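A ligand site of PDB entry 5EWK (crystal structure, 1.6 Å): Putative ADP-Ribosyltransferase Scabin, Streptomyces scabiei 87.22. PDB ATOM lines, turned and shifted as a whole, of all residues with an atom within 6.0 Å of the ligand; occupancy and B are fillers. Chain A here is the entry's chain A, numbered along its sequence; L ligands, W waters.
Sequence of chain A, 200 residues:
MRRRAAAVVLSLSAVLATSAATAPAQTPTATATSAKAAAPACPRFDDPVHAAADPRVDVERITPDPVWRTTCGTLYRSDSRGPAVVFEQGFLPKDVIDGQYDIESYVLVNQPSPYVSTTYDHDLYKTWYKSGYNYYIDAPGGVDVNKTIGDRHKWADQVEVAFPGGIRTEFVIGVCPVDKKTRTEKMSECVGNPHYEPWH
A nitrogen (N1) of the ligand sits close to the side-chain amino group (NZ) of Lys 94, 3.2 Å away. A nitrogen (N3) of the ligand is in hydrogen-bond range of the backbone carbonyl oxygen (O) of Ser 78, 2.8 Å away. The backbone NH (N) of Ser 78 sits at hydrogen-bond distance from an oxygen (O2) of the ligand (2.8 Å). ND2 of Asn 110 is in hydrogen-bond range of O1 of the ligand (2.9 Å).
CA of Arg 77 touches O2 of the ligand, 3.3 Å away. Ser 117 touches the ligand. Thr 118 touches the ligand. Thr 119 touches the ligand. Leu 124 touches the ligand. Trp 128 touches the ligand. OE1 of Gln 158 touches C10 of the ligand (3.6 Å). OE1 of Glu 160 touches C10 of the ligand, at 3.5 Å. Hydrophobic or aromatic side chains that line the ligand: Leu 124 and Trp 128. Within 4 Å of the ligand: Arg 77, Ser 78, Lys 94, Asn 110, Ser 117, Thr 118, Thr 119, Leu 124, Trp 128, Gln 158 and Glu 160. The nearest printed residue that does not touch the ligand is Tyr 76 (4.2 Å).
Water W1 lies within hydrogen-bond range of O2 of the ligand (2.8 Å), NE1 of Trp 128 (3.4 Å) and N of Ser 78 (3.4 Å). Water W5 lies within hydrogen-bond range of an oxygen (O1) of the ligand, the backbone carbonyl oxygen (O) of Gln 111 and the side-chain amide nitrogen (ND2) of Asn 110. Water W2 lies within hydrogen-bond range of OH of Tyr 106, N of Ser 117 and NH2 of Arg 77. Water W6 bridges the backbone carbonyl oxygen of Tyr 115 (2.6 Å) and the backbone NH of Lys 94 (2.9 Å).
OG1 of Thr 119 lies within hydrogen-bond range of O of Gln 158 (2.7 Å). The side-chain carboxylate (OD2) of Asp 79 lies within salt-bridge range of the guanidinium group (NE) of Arg 77 (2.8 Å). N of Val 161 is in hydrogen-bond range of O of Thr 118, at 2.8 Å. The backbone carbonyl oxygen (O) of Ser 117 is in hydrogen-bond range of the guanidinium group (NH2) of Arg 77 (2.9 Å). The side-chain hydroxyl of Thr 119 lies close to the backbone carbonyl oxygen of Val 159, 3.4 Å away. The side-chain hydroxyl (OG) of Ser 117 is in hydrogen-bond range of the side-chain hydroxyl (OH) of Tyr 106 (2.5 Å). OG of Ser 117 is in hydrogen-bond range of OE2 of Glu 160 (2.5 Å). O of Tyr 76 is in hydrogen-bond range of N of Thr 119 (2.8 Å).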
ATOM      1  N   TYR A  76      20.691  -9.069  35.491  1.00  0.00           N
ATOM      2  CA  TYR A  76      19.302  -9.252  35.888  1.00  0.00           C
ATOM      3  C   TYR A  76      18.430  -9.206  34.649  1.00  0.00           C
ATOM      4  O   TYR A  76      18.764  -8.581  33.644  1.00  0.00           O
ATOM      5  CB  TYR A  76      18.852  -8.179  36.911  1.00  0.00           C
ATOM      6  CG  TYR A  76      19.854  -8.092  38.046  1.00  0.00           C
ATOM      7  CD1 TYR A  76      20.925  -7.240  37.964  1.00  0.00           C
ATOM      8  CD2 TYR A  76      19.721  -8.880  39.139  1.00  0.00           C
ATOM      9  CE1 TYR A  76      21.888  -7.181  38.976  1.00  0.00           C
ATOM     10  CE2 TYR A  76      20.675  -8.821  40.166  1.00  0.00           C
ATOM     11  CZ  TYR A  76      21.726  -7.968  40.061  1.00  0.00           C
ATOM     12  OH  TYR A  76      22.691  -7.947  41.057  1.00  0.00           O
ATOM     13  N   ARG A  77      17.301  -9.902  34.717  1.00  0.00           N
ATOM     14  CA  ARG A  77      16.275  -9.792  33.682  1.00  0.00           C
ATOM     15  C   ARG A  77      14.901  -9.879  34.315  1.00  0.00           C
ATOM     16  O   ARG A  77      14.577 -10.871  34.976  1.00  0.00           O
ATOM     17  CB  ARG A  77      16.428 -10.883  32.609  1.00  0.00           C
ATOM     18  CG  ARG A  77      15.359 -10.806  31.534  1.00  0.00           C
ATOM     19  CD  ARG A  77      15.536 -11.875  30.433  1.00  0.00           C
ATOM     20  NE  ARG A  77      14.289 -12.018  29.676  1.00  0.00           N
ATOM     21  CZ  ARG A  77      13.914 -11.250  28.665  1.00  0.00           C
ATOM     22  NH1 ARG A  77      12.726 -11.470  28.087  1.00  0.00           N
ATOM     23  NH2 ARG A  77      14.687 -10.280  28.200  1.00  0.00           N
ATOM     24  N   SER A  78      14.109  -8.828  34.080  1.00  0.00           N
ATOM     25  CA  SER A  78      12.689  -8.798  34.382  1.00  0.00           C
ATOM     26  C   SER A  78      11.963  -9.596  33.304  1.00  0.00           C
ATOM     27  O   SER A  78      12.181  -9.364  32.106  1.00  0.00           O
ATOM     28  CB  SER A  78      12.241  -7.329  34.412  1.00  0.00           C
ATOM     29  OG  SER A  78      10.846  -7.296  34.655  1.00  0.00           O
ATOM     30  N   ASP A  79      11.152 -10.567  33.698  1.00  0.00           N
ATOM     31  CA  ASP A  79      10.435 -11.393  32.724  1.00  0.00           C
ATOM     32  C   ASP A  79       9.140 -11.880  33.350  1.00  0.00           C
ATOM     33  O   ASP A  79       9.109 -12.278  34.519  1.00  0.00           O
ATOM     34  CB  ASP A  79      11.305 -12.561  32.257  1.00  0.00           C
ATOM     35  CG  ASP A  79      10.958 -13.081  30.883  1.00  0.00           C
ATOM     36  OD1 ASP A  79       9.755 -13.158  30.535  1.00  0.00           O
ATOM     37  OD2 ASP A  79      11.896 -13.449  30.142  1.00  0.00           O
ATOM     38  N   LEU A  92      15.476 -18.078  25.736  1.00  0.00           N
ATOM     39  CA  LEU A  92      15.625 -18.196  24.290  1.00  0.00           C
ATOM     40  C   LEU A  92      15.234 -16.898  23.616  1.00  0.00           C
ATOM     41  O   LEU A  92      14.269 -16.250  24.052  1.00  0.00           O
ATOM     42  CB  LEU A  92      14.777 -19.337  23.743  1.00  0.00           C
ATOM     43  CG  LEU A  92      15.178 -20.737  24.180  1.00  0.00           C
ATOM     44  CD1 LEU A  92      14.032 -21.724  23.905  1.00  0.00           C
ATOM     45  CD2 LEU A  92      16.439 -21.177  23.436  1.00  0.00           C
ATOM     46  N   PRO A  93      15.951 -16.484  22.582  1.00  0.00           N
ATOM     47  CA  PRO A  93      15.550 -15.290  21.831  1.00  0.00           C
ATOM     48  C   PRO A  93      14.351 -15.579  20.952  1.00  0.00           C
ATOM     49  O   PRO A  93      14.079 -16.730  20.568  1.00  0.00           O
ATOM     50  CB  PRO A  93      16.781 -14.977  20.986  1.00  0.00           C
ATOM     51  CG  PRO A  93      17.345 -16.305  20.709  1.00  0.00           C
ATOM     52  CD  PRO A  93      17.131 -17.119  21.964  1.00  0.00           C
ATOM     53  N   LYS A  94      13.653 -14.503  20.595  1.00  0.00           N
ATOM     54  CA  LYS A  94      12.466 -14.626  19.757  1.00  0.00           C
ATOM     55  C   LYS A  94      12.806 -15.146  18.349  1.00  0.00           C
ATOM     56  O   LYS A  94      12.121 -16.030  17.838  1.00  0.00           O
ATOM     57  CB  LYS A  94      11.748 -13.288  19.666  1.00  0.00           C
ATOM     58  CG  LYS A  94      11.140 -12.781  20.975  1.00  0.00           C
ATOM     59  CD  LYS A  94      10.176 -11.639  20.684  1.00  0.00           C
ATOM     60  CE  LYS A  94      10.018 -10.660  21.839  1.00  0.00           C
ATOM     61  NZ  LYS A  94       8.963 -11.060  22.827  1.00  0.00           N
ATOM     62  N   TYR A 106      16.535  -2.581  17.618  1.00  0.00           N
ATOM     63  CA  TYR A 106      15.905  -3.440  18.627  1.00  0.00           C
ATOM     64  C   TYR A 106      15.574  -2.663  19.899  1.00  0.00           C
ATOM     65  O   TYR A 106      14.472  -2.779  20.467  1.00  0.00           O
ATOM     66  CB  TYR A 106      16.865  -4.609  18.937  1.00  0.00           C
ATOM     67  CG  TYR A 106      16.547  -5.401  20.195  1.00  0.00           C
ATOM     68  CD1 TYR A 106      15.406  -6.170  20.261  1.00  0.00           C
ATOM     69  CD2 TYR A 106      17.434  -5.427  21.296  1.00  0.00           C
ATOM     70  CE1 TYR A 106      15.085  -6.901  21.383  1.00  0.00           C
ATOM     71  CE2 TYR A 106      17.124  -6.162  22.425  1.00  0.00           C
ATOM     72  CZ  TYR A 106      15.942  -6.905  22.462  1.00  0.00           C
ATOM     73  OH  TYR A 106      15.558  -7.663  23.553  1.00  0.00           O
ATOM     74  N   ASN A 110      10.695  -2.132  19.747  1.00  0.00           N
ATOM     75  CA  ASN A 110      10.781  -3.532  20.119  1.00  0.00           C
ATOM     76  C   ASN A 110      10.242  -4.373  18.964  1.00  0.00           C
ATOM     77  O   ASN A 110       9.169  -4.098  18.422  1.00  0.00           O
ATOM     78  CB  ASN A 110      10.041  -3.822  21.414  1.00  0.00           C
ATOM     79  CG  ASN A 110      10.393  -5.179  22.005  1.00  0.00           C
ATOM     80  OD1 ASN A 110      11.415  -5.338  22.664  1.00  0.00           O
ATOM     81  ND2 ASN A 110       9.544  -6.168  21.748  1.00  0.00           N
ATOM     82  N   GLN A 111      11.040  -5.355  18.566  1.00  0.00           N
ATOM     83  CA  GLN A 111      10.730  -6.238  17.462  1.00  0.00           C
ATOM     84  C   GLN A 111      11.465  -7.539  17.708  1.00  0.00           C
ATOM     85  O   GLN A 111      12.462  -7.555  18.443  1.00  0.00           O
ATOM     86  CB  GLN A 111      11.155  -5.645  16.109  1.00  0.00           C
ATOM     87  CG  GLN A 111      12.563  -5.117  16.078  1.00  0.00           C
ATOM     88  CD  GLN A 111      12.747  -4.018  15.045  1.00  0.00           C
ATOM     89  OE1 GLN A 111      12.790  -4.269  13.851  1.00  0.00           O
ATOM     90  NE2 GLN A 111      12.892  -2.794  15.515  1.00  0.00           N
ATOM     91  N   TYR A 115      18.385 -11.447  20.269  1.00  0.00           N
ATOM     92  CA  TYR A 115      18.959 -11.054  21.540  1.00  0.00           C
ATOM     93  C   TYR A 115      18.014 -11.352  22.703  1.00  0.00           C
ATOM     94  O   TYR A 115      16.793 -11.198  22.593  1.00  0.00           O
ATOM     95  CB  TYR A 115      19.286  -9.550  21.540  1.00  0.00           C
ATOM     96  CG  TYR A 115      20.173  -9.132  20.418  1.00  0.00           C
ATOM     97  CD1 TYR A 115      21.512  -9.465  20.412  1.00  0.00           C
ATOM     98  CD2 TYR A 115      19.668  -8.396  19.355  1.00  0.00           C
ATOM     99  CE1 TYR A 115      22.343  -9.089  19.361  1.00  0.00           C
ATOM    100  CE2 TYR A 115      20.477  -8.000  18.311  1.00  0.00           C
ATOM    101  CZ  TYR A 115      21.816  -8.338  18.318  1.00  0.00           C
ATOM    102  OH  TYR A 115      22.640  -7.955  17.269  1.00  0.00           O
ATOM    103  N   VAL A 116      18.578 -11.756  23.829  1.00  0.00           N
ATOM    104  CA  VAL A 116      17.876 -11.690  25.102  1.00  0.00           C
ATOM    105  C   VAL A 116      18.455 -10.544  25.913  1.00  0.00           C
ATOM    106  O   VAL A 116      19.655 -10.531  26.217  1.00  0.00           O
ATOM    107  CB  VAL A 116      17.972 -13.005  25.897  1.00  0.00           C
ATOM    108  CG1 VAL A 116      17.334 -12.837  27.289  1.00  0.00           C
ATOM    109  CG2 VAL A 116      17.279 -14.150  25.111  1.00  0.00           C
ATOM    110  N   SER A 117      17.582  -9.609  26.302  1.00  0.00           N
ATOM    111  CA  SER A 117      18.005  -8.422  27.036  1.00  0.00           C
ATOM    112  C   SER A 117      18.129  -8.707  28.525  1.00  0.00           C
ATOM    113  O   SER A 117      17.259  -9.318  29.140  1.00  0.00           O
ATOM    114  CB  SER A 117      17.004  -7.284  26.856  1.00  0.00           C
ATOM    115  OG  SER A 117      16.970  -6.889  25.504  1.00  0.00           O
ATOM    116  N   THR A 118      19.230  -8.213  29.093  1.00  0.00           N
ATOM    117  CA  THR A 118      19.468  -8.202  30.533  1.00  0.00           C
ATOM    118  C   THR A 118      19.958  -6.813  30.918  1.00  0.00           C
ATOM    119  O   THR A 118      20.224  -5.963  30.053  1.00  0.00           O
ATOM    120  CB  THR A 118      20.515  -9.253  30.946  1.00  0.00           C
ATOM    121  OG1 THR A 118      21.795  -8.817  30.497  1.00  0.00           O
ATOM    122  CG2 THR A 118      20.151 -10.644  30.360  1.00  0.00           C
ATOM    123  N   THR A 119      20.136  -6.585  32.209  1.00  0.00           N
ATOM    124  CA  THR A 119      20.592  -5.308  32.714  1.00  0.00           C
ATOM    125  C   THR A 119      21.617  -5.479  33.831  1.00  0.00           C
ATOM    126  O   THR A 119      21.588  -6.447  34.598  1.00  0.00           O
ATOM    127  CB  THR A 119      19.393  -4.458  33.231  1.00  0.00           C
ATOM    128  OG1 THR A 119      19.865  -3.213  33.745  1.00  0.00           O
ATOM    129  CG2 THR A 119      18.602  -5.194  34.298  1.00  0.00           C
ATOM    130  N   LEU A 124      16.008  -2.599  37.985  1.00  0.00           N
ATOM    131  CA  LEU A 124      15.263  -2.185  36.790  1.00  0.00           C
ATOM    132  C   LEU A 124      13.890  -2.848  36.749  1.00  0.00           C
ATOM    133  O   LEU A 124      12.974  -2.320  36.110  1.00  0.00           O
ATOM    134  CB  LEU A 124      16.075  -2.529  35.526  1.00  0.00           C
ATOM    135  CG  LEU A 124      15.484  -1.831  34.263  1.00  0.00           C
ATOM    136  CD1 LEU A 124      15.713  -0.353  34.331  1.00  0.00           C
ATOM    137  CD2 LEU A 124      16.125  -2.412  33.010  1.00  0.00           C
ATOM    138  N   TRP A 128       9.275  -2.212  35.092  1.00  0.00           N
ATOM    139  CA  TRP A 128       8.501  -3.091  34.215  1.00  0.00           C
ATOM    140  C   TRP A 128       7.214  -3.455  34.950  1.00  0.00           C
ATOM    141  O   TRP A 128       7.246  -4.168  35.955  1.00  0.00           O
ATOM    142  CB  TRP A 128       9.282  -4.350  33.857  1.00  0.00           C
ATOM    143  CG  TRP A 128      10.540  -4.112  33.128  1.00  0.00           C
ATOM    144  CD1 TRP A 128      11.776  -3.949  33.670  1.00  0.00           C
ATOM    145  CD2 TRP A 128      10.703  -3.995  31.707  1.00  0.00           C
ATOM    146  NE1 TRP A 128      12.700  -3.738  32.684  1.00  0.00           N
ATOM    147  CE2 TRP A 128      12.081  -3.757  31.464  1.00  0.00           C
ATOM    148  CE3 TRP A 128       9.834  -4.059  30.614  1.00  0.00           C
ATOM    149  CZ2 TRP A 128      12.597  -3.596  30.185  1.00  0.00           C
ATOM    150  CZ3 TRP A 128      10.361  -3.903  29.341  1.00  0.00           C
ATOM    151  CH2 TRP A 128      11.723  -3.669  29.141  1.00  0.00           C
ATOM    152  N   GLN A 158      18.573   1.937  30.986  1.00  0.00           N
ATOM    153  CA  GLN A 158      18.322   0.511  31.171  1.00  0.00           C
ATOM    154  C   GLN A 158      19.608  -0.281  31.341  1.00  0.00           C
ATOM    155  O   GLN A 158      19.539  -1.466  31.703  1.00  0.00           O
ATOM    156  CB  GLN A 158      17.575  -0.089  29.985  1.00  0.00           C
ATOM    157  CG  GLN A 158      16.172   0.448  29.744  1.00  0.00           C
ATOM    158  CD  GLN A 158      15.462  -0.377  28.663  1.00  0.00           C
ATOM    159  OE1 GLN A 158      15.987  -0.569  27.540  1.00  0.00           O
ATOM    160  NE2 GLN A 158      14.291  -0.899  29.004  1.00  0.00           N
ATOM    161  N   VAL A 159      20.756   0.370  31.077  1.00  0.00           N
ATOM    162  CA  VAL A 159      22.109  -0.190  31.189  1.00  0.00           C
ATOM    163  C   VAL A 159      22.092  -1.668  30.795  1.00  0.00           C
ATOM    164  O   VAL A 159      22.419  -2.588  31.575  1.00  0.00           O
ATOM    165  CB  VAL A 159      22.696   0.078  32.592  1.00  0.00           C
ATOM    166  CG1 VAL A 159      22.969   1.573  32.748  1.00  0.00           C
ATOM    167  CG2 VAL A 159      21.783  -0.401  33.717  1.00  0.00           C
ATOM    168  N   GLU A 160      21.731  -1.880  29.538  1.00  0.00           N
ATOM    169  CA  GLU A 160      21.399  -3.180  29.008  1.00  0.00           C
ATOM    170  C   GLU A 160      22.635  -3.938  28.557  1.00  0.00           C
ATOM    171  O   GLU A 160      23.592  -3.354  28.028  1.00  0.00           O
ATOM    172  CB  GLU A 160      20.437  -3.024  27.827  1.00  0.00           C
ATOM    173  CG  GLU A 160      19.997  -4.326  27.228  1.00  0.00           C
ATOM    174  CD  GLU A 160      19.055  -4.175  26.038  1.00  0.00           C
ATOM    175  OE1 GLU A 160      18.516  -3.067  25.821  1.00  0.00           O
ATOM    176  OE2 GLU A 160      18.855  -5.192  25.338  1.00  0.00           O
ATOM    177  N   VAL A 161      22.592  -5.258  28.739  1.00  0.00           N
ATOM    178  CA  VAL A 161      23.518  -6.206  28.131  1.00  0.00           C
ATOM    179  C   VAL A 161      22.660  -7.168  27.314  1.00  0.00           C
ATOM    180  O   VAL A 161      21.737  -7.796  27.856  1.00  0.00           O
ATOM    181  CB  VAL A 161      24.370  -6.940  29.186  1.00  0.00           C
ATOM    182  CG1 VAL A 161      25.267  -7.982  28.498  1.00  0.00           C
ATOM    183  CG2 VAL A 161      25.188  -5.942  29.994  1.00  0.00           C
HETATM  184  C1  LIG L   1      12.751 -11.560  24.723  1.00  0.00           C
HETATM  185  N1  LIG L   1      11.573 -10.700  24.690  1.00  0.00           N
HETATM  186  C2  LIG L   1      10.529 -11.323  25.443  1.00  0.00           C
HETATM  187  C3  LIG L   1      11.881  -9.422  25.293  1.00  0.00           C
HETATM  188  C4  LIG L   1      11.211  -8.120  24.820  1.00  0.00           C
HETATM  189  O1  LIG L   1      10.635  -8.059  23.722  1.00  0.00           O
HETATM  190  N2  LIG L   1      11.340  -7.010  25.640  1.00  0.00           N
HETATM  191  C5  LIG L   1      11.980  -7.062  26.908  1.00  0.00           C
HETATM  192  C6  LIG L   1      13.084  -6.260  27.186  1.00  0.00           C
HETATM  193  C7  LIG L   1      13.687  -6.387  28.465  1.00  0.00           C
HETATM  194  C8  LIG L   1      14.854  -5.591  28.906  1.00  0.00           C
HETATM  195  C9  LIG L   1      15.479  -4.666  28.080  1.00  0.00           C
HETATM  196  C10 LIG L   1      16.562  -3.952  28.534  1.00  0.00           C
HETATM  197  C11 LIG L   1      17.096  -4.167  29.809  1.00  0.00           C
HETATM  198  C12 LIG L   1      16.484  -5.111  30.643  1.00  0.00           C
HETATM  199  C13 LIG L   1      15.382  -5.820  30.198  1.00  0.00           C
HETATM  200  C14 LIG L   1      14.761  -6.751  31.138  1.00  0.00           C
HETATM  201  O2  LIG L   1      15.190  -6.970  32.274  1.00  0.00           O
HETATM  202  N3  LIG L   1      13.700  -7.455  30.681  1.00  0.00           N
HETATM  203  C15 LIG L   1      13.146  -7.282  29.379  1.00  0.00           C
HETATM  204  C16 LIG L   1      12.040  -8.074  29.067  1.00  0.00           C
HETATM  205  C17 LIG L   1      11.473  -7.928  27.845  1.00  0.00           C
HETATM  206  O   HOH W   1      14.861  -5.515  34.666  1.00  0.00           O
HETATM  207  O   HOH W   2      14.865  -9.645  25.275  1.00  0.00           O
HETATM  208  O   HOH W   3      10.180 -14.389  26.061  1.00  0.00           O
HETATM  209  O   HOH W   4       8.806 -12.475  28.078  1.00  0.00           O
HETATM  210  O   HOH W   5      11.618  -8.501  21.099  1.00  0.00           O
HETATM  211  O   HOH W   6      14.392 -12.202  22.201  1.00  0.00           O
